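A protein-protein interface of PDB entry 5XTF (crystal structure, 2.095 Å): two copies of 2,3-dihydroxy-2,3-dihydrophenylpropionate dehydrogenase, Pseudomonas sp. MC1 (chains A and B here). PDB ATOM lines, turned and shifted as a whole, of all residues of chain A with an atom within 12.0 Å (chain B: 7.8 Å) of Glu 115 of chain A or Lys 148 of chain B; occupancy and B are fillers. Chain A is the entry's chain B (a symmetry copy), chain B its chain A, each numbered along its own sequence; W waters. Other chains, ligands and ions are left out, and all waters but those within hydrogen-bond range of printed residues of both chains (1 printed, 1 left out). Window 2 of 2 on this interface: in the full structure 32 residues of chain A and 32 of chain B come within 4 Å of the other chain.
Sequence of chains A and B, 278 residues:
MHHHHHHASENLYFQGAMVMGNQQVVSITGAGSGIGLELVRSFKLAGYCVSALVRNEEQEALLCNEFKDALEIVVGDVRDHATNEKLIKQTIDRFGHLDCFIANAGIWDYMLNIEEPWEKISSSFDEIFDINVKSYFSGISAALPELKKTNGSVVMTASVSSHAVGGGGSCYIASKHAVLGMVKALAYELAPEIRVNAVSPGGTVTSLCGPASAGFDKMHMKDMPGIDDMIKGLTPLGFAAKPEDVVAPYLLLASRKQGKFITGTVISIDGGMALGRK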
ATOM      1  N   ASP A 109     -11.382  10.711  26.473  1.00  0.00           N
ATOM      2  CA  ASP A 109     -11.147  11.928  25.707  1.00  0.00           C
ATOM      3  C   ASP A 109     -10.330  12.973  26.453  1.00  0.00           C
ATOM      4  O   ASP A 109     -10.142  14.072  25.927  1.00  0.00           O
ATOM      5  CB  ASP A 109     -12.475  12.541  25.239  1.00  0.00           C
ATOM      6  CG  ASP A 109     -13.246  13.246  26.346  1.00  0.00           C
ATOM      7  OD1 ASP A 109     -12.924  13.070  27.550  1.00  0.00           O
ATOM      8  OD2 ASP A 109     -14.219  13.965  25.989  1.00  0.00           O
ATOM      9  N   TYR A 110      -9.846  12.666  27.658  1.00  0.00           N
ATOM     10  CA  TYR A 110      -8.924  13.540  28.387  1.00  0.00           C
ATOM     11  C   TYR A 110      -9.488  14.957  28.517  1.00  0.00           C
ATOM     12  O   TYR A 110      -8.790  15.952  28.306  1.00  0.00           O
ATOM     13  CB  TYR A 110      -7.535  13.536  27.728  1.00  0.00           C
ATOM     14  CG  TYR A 110      -6.912  12.151  27.705  1.00  0.00           C
ATOM     15  CD1 TYR A 110      -6.067  11.727  28.728  1.00  0.00           C
ATOM     16  CD2 TYR A 110      -7.197  11.250  26.680  1.00  0.00           C
ATOM     17  CE1 TYR A 110      -5.513  10.452  28.724  1.00  0.00           C
ATOM     18  CE2 TYR A 110      -6.647   9.969  26.668  1.00  0.00           C
ATOM     19  CZ  TYR A 110      -5.806   9.581  27.693  1.00  0.00           C
ATOM     20  OH  TYR A 110      -5.253   8.324  27.689  1.00  0.00           O
ATOM     21  N   MET A 111     -10.779  15.032  28.852  1.00  0.00           N
ATOM     22  CA  MET A 111     -11.480  16.282  29.162  1.00  0.00           C
ATOM     23  C   MET A 111     -11.408  17.298  28.020  1.00  0.00           C
ATOM     24  O   MET A 111     -11.379  18.510  28.265  1.00  0.00           O
ATOM     25  CB  MET A 111     -10.955  16.909  30.462  1.00  0.00           C
ATOM     26  CG  MET A 111     -10.739  15.930  31.613  1.00  0.00           C
ATOM     27  SD  MET A 111     -12.253  15.124  32.182  1.00  0.00           S
ATOM     28  CE  MET A 111     -13.230  16.543  32.714  1.00  0.00           C
ATOM     29  N   LEU A 112     -11.398  16.819  26.773  1.00  0.00           N
ATOM     30  CA  LEU A 112     -11.353  17.698  25.608  1.00  0.00           C
ATOM     31  C   LEU A 112     -12.435  18.772  25.693  1.00  0.00           C
ATOM     32  O   LEU A 112     -13.621  18.456  25.806  1.00  0.00           O
ATOM     33  CB  LEU A 112     -11.522  16.863  24.335  1.00  0.00           C
ATOM     34  CG  LEU A 112     -11.599  17.692  23.051  1.00  0.00           C
ATOM     35  CD1 LEU A 112     -10.298  18.448  22.831  1.00  0.00           C
ATOM     36  CD2 LEU A 112     -11.942  16.848  21.844  1.00  0.00           C
ATOM     37  N   ASN A 113     -12.023  20.043  25.661  1.00  0.00           N
ATOM     38  CA  ASN A 113     -12.955  21.163  25.782  1.00  0.00           C
ATOM     39  C   ASN A 113     -13.636  21.474  24.457  1.00  0.00           C
ATOM     40  O   ASN A 113     -13.062  21.304  23.382  1.00  0.00           O
ATOM     41  CB  ASN A 113     -12.248  22.423  26.273  1.00  0.00           C
ATOM     42  CG  ASN A 113     -11.883  22.347  27.735  1.00  0.00           C
ATOM     43  OD1 ASN A 113     -12.739  22.479  28.609  1.00  0.00           O
ATOM     44  ND2 ASN A 113     -10.603  22.131  28.014  1.00  0.00           N
ATOM     45  N   ILE A 114     -14.872  21.966  24.550  1.00  0.00           N
ATOM     46  CA  ILE A 114     -15.630  22.299  23.354  1.00  0.00           C
ATOM     47  C   ILE A 114     -15.110  23.572  22.690  1.00  0.00           C
ATOM     48  O   ILE A 114     -15.436  23.826  21.526  1.00  0.00           O
ATOM     49  CB  ILE A 114     -17.125  22.417  23.711  1.00  0.00           C
ATOM     50  CG1 ILE A 114     -17.999  22.526  22.444  1.00  0.00           C
ATOM     51  CG2 ILE A 114     -17.351  23.588  24.674  1.00  0.00           C
ATOM     52  CD1 ILE A 114     -18.062  21.246  21.607  1.00  0.00           C
ATOM     53  N   GLU A 115     -14.296  24.371  23.390  1.00  0.00           N
ATOM     54  CA  GLU A 115     -13.684  25.554  22.791  1.00  0.00           C
ATOM     55  C   GLU A 115     -12.535  25.227  21.842  1.00  0.00           C
ATOM     56  O   GLU A 115     -12.176  26.069  21.017  1.00  0.00           O
ATOM     57  CB  GLU A 115     -13.161  26.497  23.874  1.00  0.00           C
ATOM     58  CG  GLU A 115     -14.246  27.247  24.640  1.00  0.00           C
ATOM     59  CD  GLU A 115     -14.257  26.896  26.113  1.00  0.00           C
ATOM     60  OE1 GLU A 115     -15.130  27.426  26.850  1.00  0.00           O
ATOM     61  OE2 GLU A 115     -13.385  26.082  26.523  1.00  0.00           O
ATOM     62  N   GLU A 116     -11.956  24.038  21.936  1.00  0.00           N
ATOM     63  CA  GLU A 116     -10.806  23.667  21.124  1.00  0.00           C
ATOM     64  C   GLU A 116     -11.114  23.790  19.634  1.00  0.00           C
ATOM     65  O   GLU A 116     -12.276  23.734  19.225  1.00  0.00           O
ATOM     66  CB  GLU A 116     -10.390  22.230  21.438  1.00  0.00           C
ATOM     67  CG  GLU A 116     -10.092  21.993  22.899  1.00  0.00           C
ATOM     68  CD  GLU A 116      -8.715  22.478  23.308  1.00  0.00           C
ATOM     69  OE1 GLU A 116      -7.712  21.923  22.796  1.00  0.00           O
ATOM     70  OE2 GLU A 116      -8.644  23.411  24.144  1.00  0.00           O
ATOM     71  N   PRO A 117     -10.076  23.950  18.806  1.00  0.00           N
ATOM     72  CA  PRO A 117     -10.289  24.038  17.354  1.00  0.00           C
ATOM     73  C   PRO A 117     -10.976  22.801  16.794  1.00  0.00           C
ATOM     74  O   PRO A 117     -10.656  21.667  17.161  1.00  0.00           O
ATOM     75  CB  PRO A 117      -8.868  24.195  16.797  1.00  0.00           C
ATOM     76  CG  PRO A 117      -7.946  23.923  17.944  1.00  0.00           C
ATOM     77  CD  PRO A 117      -8.692  24.286  19.171  1.00  0.00           C
ATOM     78  N   TRP A 118     -11.920  23.036  15.878  1.00  0.00           N
ATOM     79  CA  TRP A 118     -12.791  21.965  15.405  1.00  0.00           C
ATOM     80  C   TRP A 118     -12.003  20.786  14.851  1.00  0.00           C
ATOM     81  O   TRP A 118     -12.425  19.635  15.001  1.00  0.00           O
ATOM     82  CB  TRP A 118     -13.763  22.500  14.354  1.00  0.00           C
ATOM     83  CG  TRP A 118     -14.578  21.418  13.728  1.00  0.00           C
ATOM     84  CD1 TRP A 118     -14.498  20.965  12.446  1.00  0.00           C
ATOM     85  CD2 TRP A 118     -15.580  20.626  14.375  1.00  0.00           C
ATOM     86  NE1 TRP A 118     -15.400  19.943  12.246  1.00  0.00           N
ATOM     87  CE2 TRP A 118     -16.078  19.717  13.415  1.00  0.00           C
ATOM     88  CE3 TRP A 118     -16.113  20.603  15.672  1.00  0.00           C
ATOM     89  CZ2 TRP A 118     -17.076  18.787  13.711  1.00  0.00           C
ATOM     90  CZ3 TRP A 118     -17.110  19.677  15.968  1.00  0.00           C
ATOM     91  CH2 TRP A 118     -17.580  18.782  14.990  1.00  0.00           C
ATOM     92  N   GLU A 119     -10.859  21.045  14.221  1.00  0.00           N
ATOM     93  CA  GLU A 119     -10.034  19.972  13.679  1.00  0.00           C
ATOM     94  C   GLU A 119      -9.738  18.928  14.743  1.00  0.00           C
ATOM     95  O   GLU A 119      -9.819  17.717  14.488  1.00  0.00           O
ATOM     96  CB  GLU A 119      -8.738  20.557  13.117  1.00  0.00           C
ATOM     97  CG  GLU A 119      -8.919  21.576  11.962  1.00  0.00           C
ATOM     98  CD  GLU A 119      -9.758  22.816  12.314  1.00  0.00           C
ATOM     99  OE1 GLU A 119     -10.312  23.458  11.406  1.00  0.00           O
ATOM    100  OE2 GLU A 119      -9.881  23.169  13.500  1.00  0.00           O
ATOM    101  N   LYS A 120      -9.430  19.388  15.955  1.00  0.00           N
ATOM    102  CA  LYS A 120      -9.162  18.486  17.062  1.00  0.00           C
ATOM    103  C   LYS A 120     -10.438  17.819  17.556  1.00  0.00           C
ATOM    104  O   LYS A 120     -10.453  16.604  17.806  1.00  0.00           O
ATOM    105  CB  LYS A 120      -8.471  19.251  18.181  1.00  0.00           C
ATOM    106  CG  LYS A 120      -8.464  18.514  19.500  1.00  0.00           C
ATOM    107  CD  LYS A 120      -7.112  18.653  20.224  1.00  0.00           C
ATOM    108  CE  LYS A 120      -6.998  17.687  21.441  1.00  0.00           C
ATOM    109  NZ  LYS A 120      -7.232  16.230  21.111  1.00  0.00           N
ATOM    110  N   ILE A 121     -11.521  18.587  17.697  1.00  0.00           N
ATOM    111  CA  ILE A 121     -12.784  18.002  18.132  1.00  0.00           C
ATOM    112  C   ILE A 121     -13.231  16.928  17.152  1.00  0.00           C
ATOM    113  O   ILE A 121     -13.641  15.830  17.551  1.00  0.00           O
ATOM    114  CB  ILE A 121     -13.863  19.081  18.280  1.00  0.00           C
ATOM    115  CG1 ILE A 121     -13.474  20.093  19.346  1.00  0.00           C
ATOM    116  CG2 ILE A 121     -15.184  18.436  18.624  1.00  0.00           C
ATOM    117  CD1 ILE A 121     -14.456  21.214  19.428  1.00  0.00           C
ATOM    118  N   SER A 122     -13.149  17.230  15.853  1.00  0.00           N
ATOM    119  CA  SER A 122     -13.604  16.289  14.841  1.00  0.00           C
ATOM    120  C   SER A 122     -12.818  14.988  14.893  1.00  0.00           C
ATOM    121  O   SER A 122     -13.389  13.907  14.724  1.00  0.00           O
ATOM    122  CB  SER A 122     -13.485  16.904  13.456  1.00  0.00           C
ATOM    123  OG  SER A 122     -14.084  16.050  12.505  1.00  0.00           O
ATOM    124  N   SER A 124     -11.058  13.660  17.581  1.00  0.00           N
ATOM    125  CA  SER A 124     -11.392  12.952  18.805  1.00  0.00           C
ATOM    126  C   SER A 124     -12.774  12.330  18.711  1.00  0.00           C
ATOM    127  O   SER A 124     -12.964  11.168  19.101  1.00  0.00           O
ATOM    128  CB  SER A 124     -11.318  13.907  19.992  1.00  0.00           C
ATOM    129  OG  SER A 124     -10.041  14.526  20.051  1.00  0.00           O
ATOM    130  N   GLY A 168     -15.225  13.333  32.328  1.00  0.00           N
ATOM    131  CA  GLY A 168     -14.867  13.364  30.920  1.00  0.00           C
ATOM    132  C   GLY A 168     -15.322  14.659  30.273  1.00  0.00           C
ATOM    133  O   GLY A 168     -16.042  15.470  30.870  1.00  0.00           O
ATOM    134  N   GLY A 169     -14.860  14.853  29.038  1.00  0.00           N
ATOM    135  CA  GLY A 169     -15.372  15.898  28.183  1.00  0.00           C
ATOM    136  C   GLY A 169     -16.688  15.491  27.564  1.00  0.00           C
ATOM    137  O   GLY A 169     -17.247  14.429  27.838  1.00  0.00           O
ATOM    138  N   SER A 170     -17.188  16.355  26.690  1.00  0.00           N
ATOM    139  CA  SER A 170     -18.530  16.140  26.171  1.00  0.00           C
ATOM    140  C   SER A 170     -18.575  14.997  25.174  1.00  0.00           C
ATOM    141  O   SER A 170     -19.595  14.306  25.087  1.00  0.00           O
ATOM    142  CB  SER A 170     -19.059  17.424  25.539  1.00  0.00           C
ATOM    143  OG  SER A 170     -18.226  17.830  24.469  1.00  0.00           O
ATOM    144  N   CYS A 171     -17.500  14.780  24.406  1.00  0.00           N
ATOM    145  CA  CYS A 171     -17.483  13.621  23.514  1.00  0.00           C
ATOM    146  C   CYS A 171     -17.610  12.331  24.309  1.00  0.00           C
ATOM    147  O   CYS A 171     -18.480  11.498  24.028  1.00  0.00           O
ATOM    148  CB  CYS A 171     -16.207  13.594  22.671  1.00  0.00           C
ATOM    149  SG  CYS A 171     -16.012  15.057  21.627  1.00  0.00           S
ATOM    150  N   LEU B  98     -25.270  36.959  17.975  1.00  0.00           N
ATOM    151  CA  LEU B  98     -26.062  35.735  18.045  1.00  0.00           C
ATOM    152  C   LEU B  98     -26.424  35.485  19.496  1.00  0.00           C
ATOM    153  O   LEU B  98     -25.538  35.459  20.353  1.00  0.00           O
ATOM    154  CB  LEU B  98     -25.310  34.525  17.476  1.00  0.00           C
ATOM    155  CG  LEU B  98     -26.076  33.201  17.533  1.00  0.00           C
ATOM    156  CD1 LEU B  98     -27.310  33.219  16.624  1.00  0.00           C
ATOM    157  CD2 LEU B  98     -25.162  32.038  17.179  1.00  0.00           C
ATOM    158  N   ILE B 140     -22.395  23.852  17.361  1.00  0.00           N
ATOM    159  CA  ILE B 140     -22.120  24.547  18.615  1.00  0.00           C
ATOM    160  C   ILE B 140     -20.688  25.066  18.643  1.00  0.00           C
ATOM    161  O   ILE B 140     -20.416  26.145  19.182  1.00  0.00           O
ATOM    162  CB  ILE B 140     -22.401  23.613  19.810  1.00  0.00           C
ATOM    163  CG1 ILE B 140     -23.907  23.387  19.986  1.00  0.00           C
ATOM    164  CG2 ILE B 140     -21.751  24.146  21.097  1.00  0.00           C
ATOM    165  CD1 ILE B 140     -24.194  22.065  20.725  1.00  0.00           C
ATOM    166  N   SER B 141     -19.740  24.281  18.135  1.00  0.00           N
ATOM    167  CA  SER B 141     -18.377  24.786  18.001  1.00  0.00           C
ATOM    168  C   SER B 141     -18.348  26.051  17.150  1.00  0.00           C
ATOM    169  O   SER B 141     -17.685  27.037  17.493  1.00  0.00           O
ATOM    170  CB  SER B 141     -17.484  23.708  17.385  1.00  0.00           C
ATOM    171  OG  SER B 141     -16.160  24.183  17.198  1.00  0.00           O
ATOM    172  N   ALA B 143     -20.794  28.155  16.707  1.00  0.00           N
ATOM    173  CA  ALA B 143     -21.571  29.226  17.319  1.00  0.00           C
ATOM    174  C   ALA B 143     -20.989  29.724  18.635  1.00  0.00           C
ATOM    175  O   ALA B 143     -21.391  30.792  19.101  1.00  0.00           O
ATOM    176  CB  ALA B 143     -23.014  28.762  17.552  1.00  0.00           C
ATOM    177  N   LEU B 144     -20.059  28.984  19.234  1.00  0.00           N
ATOM    178  CA  LEU B 144     -19.621  29.281  20.600  1.00  0.00           C
ATOM    179  C   LEU B 144     -18.999  30.666  20.774  1.00  0.00           C
ATOM    180  O   LEU B 144     -19.366  31.357  21.742  1.00  0.00           O
ATOM    181  CB  LEU B 144     -18.659  28.180  21.066  1.00  0.00           C
ATOM    182  CG  LEU B 144     -18.173  28.143  22.524  1.00  0.00           C
ATOM    183  CD1 LEU B 144     -19.302  27.940  23.482  1.00  0.00           C
ATOM    184  CD2 LEU B 144     -17.171  27.001  22.668  1.00  0.00           C
ATOM    185  N   PRO B 145     -18.053  31.124  19.937  1.00  0.00           N
ATOM    186  CA  PRO B 145     -17.423  32.425  20.226  1.00  0.00           C
ATOM    187  C   PRO B 145     -18.416  33.565  20.251  1.00  0.00           C
ATOM    188  O   PRO B 145     -18.228  34.530  21.000  1.00  0.00           O
ATOM    189  CB  PRO B 145     -16.403  32.588  19.088  1.00  0.00           C
ATOM    190  CG  PRO B 145     -16.099  31.210  18.637  1.00  0.00           C
ATOM    191  CD  PRO B 145     -17.400  30.458  18.790  1.00  0.00           C
ATOM    192  N   GLU B 146     -19.491  33.472  19.472  1.00  0.00           N
ATOM    193  CA  GLU B 146     -20.491  34.534  19.481  1.00  0.00           C
ATOM    194  C   GLU B 146     -21.455  34.391  20.647  1.00  0.00           C
ATOM    195  O   GLU B 146     -21.910  35.399  21.187  1.00  0.00           O
ATOM    196  CB  GLU B 146     -21.254  34.539  18.165  1.00  0.00           C
ATOM    197  CG  GLU B 146     -20.385  34.938  16.977  1.00  0.00           C
ATOM    198  CD  GLU B 146     -20.048  36.438  16.949  1.00  0.00           C
ATOM    199  OE1 GLU B 146     -20.832  37.270  17.488  1.00  0.00           O
ATOM    200  OE2 GLU B 146     -18.996  36.791  16.367  1.00  0.00           O
ATOM    201  N   LEU B 147     -21.764  33.154  21.058  1.00  0.00           N
ATOM    202  CA  LEU B 147     -22.617  32.966  22.226  1.00  0.00           C
ATOM    203  C   LEU B 147     -21.935  33.449  23.498  1.00  0.00           C
ATOM    204  O   LEU B 147     -22.614  33.903  24.419  1.00  0.00           O
ATOM    205  CB  LEU B 147     -23.034  31.496  22.348  1.00  0.00           C
ATOM    206  CG  LEU B 147     -23.948  31.038  21.208  1.00  0.00           C
ATOM    207  CD1 LEU B 147     -24.096  29.519  21.171  1.00  0.00           C
ATOM    208  CD2 LEU B 147     -25.313  31.708  21.281  1.00  0.00           C
ATOM    209  N   LYS B 148     -20.604  33.390  23.562  1.00  0.00           N
ATOM    210  CA  LYS B 148     -19.904  33.868  24.753  1.00  0.00           C
ATOM    211  C   LYS B 148     -20.027  35.383  24.929  1.00  0.00           C
ATOM    212  O   LYS B 148     -20.083  35.876  26.071  1.00  0.00           O
ATOM    213  CB  LYS B 148     -18.433  33.452  24.685  1.00  0.00           C
ATOM    214  CG  LYS B 148     -18.183  31.954  24.908  1.00  0.00           C
ATOM    215  CD  LYS B 148     -16.692  31.646  24.911  1.00  0.00           C
ATOM    216  CE  LYS B 148     -16.366  30.374  25.702  1.00  0.00           C
ATOM    217  NZ  LYS B 148     -14.902  30.296  26.000  1.00  0.00           N
ATOM    218  N   LYS B 149     -20.066  36.130  23.810  1.00  0.00           N
ATOM    219  CA  LYS B 149     -20.166  37.590  23.851  1.00  0.00           C
ATOM    220  C   LYS B 149     -21.560  38.048  24.247  1.00  0.00           C
ATOM    221  O   LYS B 149     -21.721  39.146  24.785  1.00  0.00           O
ATOM    222  CB  LYS B 149     -19.788  38.192  22.490  1.00  0.00           C
ATOM    223  CG  LYS B 149     -18.355  37.878  22.054  1.00  0.00           C
ATOM    224  CD  LYS B 149     -17.860  38.783  20.925  1.00  0.00           C
ATOM    225  CE  LYS B 149     -18.332  38.313  19.556  1.00  0.00           C
ATOM    226  NZ  LYS B 149     -17.645  39.065  18.439  1.00  0.00           N
ATOM    227  N   THR B 150     -22.578  37.245  23.984  1.00  0.00           N
ATOM    228  CA  THR B 150     -23.921  37.574  24.430  1.00  0.00           C
ATOM    229  C   THR B 150     -24.332  36.786  25.663  1.00  0.00           C
ATOM    230  O   THR B 150     -25.431  37.015  26.184  1.00  0.00           O
ATOM    231  CB  THR B 150     -24.925  37.310  23.315  1.00  0.00           C
ATOM    232  OG1 THR B 150     -24.817  35.931  22.913  1.00  0.00           O
ATOM    233  CG2 THR B 150     -24.643  38.228  22.126  1.00  0.00           C
ATOM    234  N   ASN B 151     -23.475  35.876  26.141  1.00  0.00           N
ATOM    235  CA  ASN B 151     -23.856  34.888  27.140  1.00  0.00           C
ATOM    236  C   ASN B 151     -25.202  34.270  26.751  1.00  0.00           C
ATOM    237  O   ASN B 151     -26.202  34.326  27.470  1.00  0.00           O
ATOM    238  CB  ASN B 151     -23.888  35.516  28.531  1.00  0.00           C
ATOM    239  CG  ASN B 151     -22.493  35.893  29.055  1.00  0.00           C
ATOM    240  OD1 ASN B 151     -21.459  35.923  28.331  1.00  0.00           O
ATOM    241  ND2 ASN B 151     -22.463  36.188  30.337  1.00  0.00           N
ATOM    242  N   GLY B 152     -25.216  33.702  25.561  1.00  0.00           N
ATOM    243  CA  GLY B 152     -26.419  33.158  24.981  1.00  0.00           C
ATOM    244  C   GLY B 152     -26.661  31.728  25.393  1.00  0.00           C
ATOM    245  O   GLY B 152     -26.130  31.236  26.392  1.00  0.00           O
ATOM    246  N   SER B 153     -27.463  31.041  24.586  1.00  0.00           N
ATOM    247  CA  SER B 153     -27.926  29.714  24.949  1.00  0.00           C
ATOM    248  C   SER B 153     -27.966  28.817  23.724  1.00  0.00           C
ATOM    249  O   SER B 153     -28.036  29.280  22.584  1.00  0.00           O
ATOM    250  CB  SER B 153     -29.319  29.772  25.598  1.00  0.00           C
ATOM    251  OG  SER B 153     -30.256  30.385  24.716  1.00  0.00           O
ATOM    252  N   LEU B 186     -22.296  19.743  28.204  1.00  0.00           N
ATOM    253  CA  LEU B 186     -22.058  21.111  27.749  1.00  0.00           C
ATOM    254  C   LEU B 186     -22.643  22.132  28.712  1.00  0.00           C
ATOM    255  O   LEU B 186     -22.021  23.169  28.971  1.00  0.00           O
ATOM    256  CB  LEU B 186     -22.628  21.307  26.346  1.00  0.00           C
ATOM    257  CG  LEU B 186     -21.851  20.428  25.347  1.00  0.00           C
ATOM    258  CD1 LEU B 186     -22.481  20.486  23.982  1.00  0.00           C
ATOM    259  CD2 LEU B 186     -20.362  20.795  25.294  1.00  0.00           C
ATOM    260  N   GLU B 189     -20.010  22.300  31.442  1.00  0.00           N
ATOM    261  CA  GLU B 189     -18.769  22.925  30.997  1.00  0.00           C
ATOM    262  C   GLU B 189     -18.943  24.423  30.725  1.00  0.00           C
ATOM    263  O   GLU B 189     -18.053  25.219  31.035  1.00  0.00           O
ATOM    264  CB  GLU B 189     -18.262  22.212  29.747  1.00  0.00           C
ATOM    265  CG  GLU B 189     -17.069  22.858  29.120  1.00  0.00           C
ATOM    266  CD  GLU B 189     -16.511  22.046  27.966  1.00  0.00           C
ATOM    267  OE1 GLU B 189     -15.658  22.590  27.233  1.00  0.00           O
ATOM    268  OE2 GLU B 189     -16.924  20.876  27.788  1.00  0.00           O
ATOM    269  N   LEU B 190     -20.077  24.825  30.145  1.00  0.00           N
ATOM    270  CA  LEU B 190     -20.236  26.191  29.650  1.00  0.00           C
ATOM    271  C   LEU B 190     -20.886  27.141  30.646  1.00  0.00           C
ATOM    272  O   LEU B 190     -20.823  28.349  30.438  1.00  0.00           O
ATOM    273  CB  LEU B 190     -21.053  26.192  28.356  1.00  0.00           C
ATOM    274  CG  LEU B 190     -20.298  25.444  27.263  1.00  0.00           C
ATOM    275  CD1 LEU B 190     -21.146  25.353  26.021  1.00  0.00           C
ATOM    276  CD2 LEU B 190     -18.944  26.122  26.980  1.00  0.00           C
ATOM    277  N   GLU B 193     -21.805  30.946  31.799  1.00  0.00           N
ATOM    278  CA  GLU B 193     -21.920  31.893  30.692  1.00  0.00           C
ATOM    279  C   GLU B 193     -23.018  31.519  29.695  1.00  0.00           C
ATOM    280  O   GLU B 193     -23.767  32.389  29.234  1.00  0.00           O
ATOM    281  CB  GLU B 193     -20.576  32.009  29.970  1.00  0.00           C
ATOM    282  CG  GLU B 193     -20.336  33.416  29.466  1.00  0.00           C
ATOM    283  CD  GLU B 193     -19.031  33.608  28.701  1.00  0.00           C
ATOM    284  OE1 GLU B 193     -18.268  32.605  28.562  1.00  0.00           O
ATOM    285  OE2 GLU B 193     -18.804  34.768  28.241  1.00  0.00           O
ATOM    286  N   ILE B 194     -23.115  30.247  29.332  1.00  0.00           N
ATOM    287  CA  ILE B 194     -23.972  29.784  28.252  1.00  0.00           C
ATOM    288  C   ILE B 194     -24.869  28.675  28.790  1.00  0.00           C
ATOM    289  O   ILE B 194     -24.382  27.724  29.412  1.00  0.00           O
ATOM    290  CB  ILE B 194     -23.124  29.282  27.070  1.00  0.00           C
ATOM    291  CG1 ILE B 194     -22.284  30.433  26.512  1.00  0.00           C
ATOM    292  CG2 ILE B 194     -23.988  28.642  26.001  1.00  0.00           C
ATOM    293  CD1 ILE B 194     -21.383  30.047  25.388  1.00  0.00           C
HETATM  294  O   HOH W   1     -16.244  19.073  26.072  1.00  0.00           O
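Hydrophobic or aromatic side chains of chain A within 4 Å of the printed part of chain B: Ile 114 and Trp 118. Along chain B the printed residues that touch a printed residue of chain A span positions 141 to 190. Among the printed residues, 9 pairs touch across the chains. Among the printed residues, Asp or Glu carboxylates within 4 Å of a Lys or Arg side-chain nitrogen of the other chain: Glu 115 of chain A with Lys 148 of chain B.
NZ of Lys 148 of chain B is in salt-bridge range of OE1 of Glu 115 of chain A (3.0 Å). OE1 of Glu 189 of chain B sits close to OD1 of Asn 113 of chain A (3.2 Å). The side-chain carboxylate of Glu 189 of chain B sits at hydrogen-bond distance from the backbone NH of Ile 114 of chain A, at 2.9 Å.
No position is printed for both chains.
Water W1 lies within hydrogen-bond range of OE2 of Glu 189 of chain B, O of Leu 112 of chain A and OG of Ser 170 of chain A.
Tyr 110 of chain A touches none of the printed residues of chain B. Of the printed residues of chain B, Asn 113 of chain A touches Glu 189 (3.2 Å). Printed residues of chain B within 4 Å of Ile 114 of chain A: Leu 144 (3.8 Å), Leu 186 (3.95 Å), Glu 189 (2.9 Å) and Leu 190 (3.8 Å). Of chain B, only Leu 144 and Lys 148 come within 4 Å of Glu 115 of chain A. Of the printed residues of chain B, Trp 118 of chain A touches Ser 141 (3.8 Å). Ser 141 of chain B touches just one residue of chain A: Trp 118. Lys 148 of chain B touches just one residue of chain A: Glu 115. Ser 153 of chain B touches none of the printed residues of chain A. Printed residues of chain A within 4 Å of Leu 186 of chain B: Ile 114 and Ser 170. Printed residues of chain A within 4 Å of Glu 189 of chain B: Asn 113 (3.2 Å) and Ile 114 (2.9 Å). No residue of chain A comes within 4 Å of Glu 193 of chain B. The nearest residue of chain A that does not touch Lys 148 of chain B is Ile 114 of chain A (6.9 Å). The nearest printed residue of chain B that does not touch Ile 114 of chain A is Ile 140 of chain B (4.3 Å).
O of Ile 114 of chain A touches CD2 of Leu 144 of chain B, 3.8 Å away. CD2 of Leu 186 of chain B touches CB of Ile 114 of chain A (3.95 Å). Ile 114 of chain A touches Leu 190 of chain B (CG2 to CD2, 3.8 Å). CG of Glu 115 of chain A touches CD2 of Leu 144 of chain B, at 3.5 Å. CB of Ser 141 of chain B touches CE3 of Trp 118 of chain A, 3.8 Å away. Leu 186 of chain B touches Ser 170 of chain A.
The side-chain amide oxygen (OD1) of Asn 151 of chain B lies close to the backbone carbonyl oxygen (O) of Lys 148 of chain B, at 2.6 Å.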
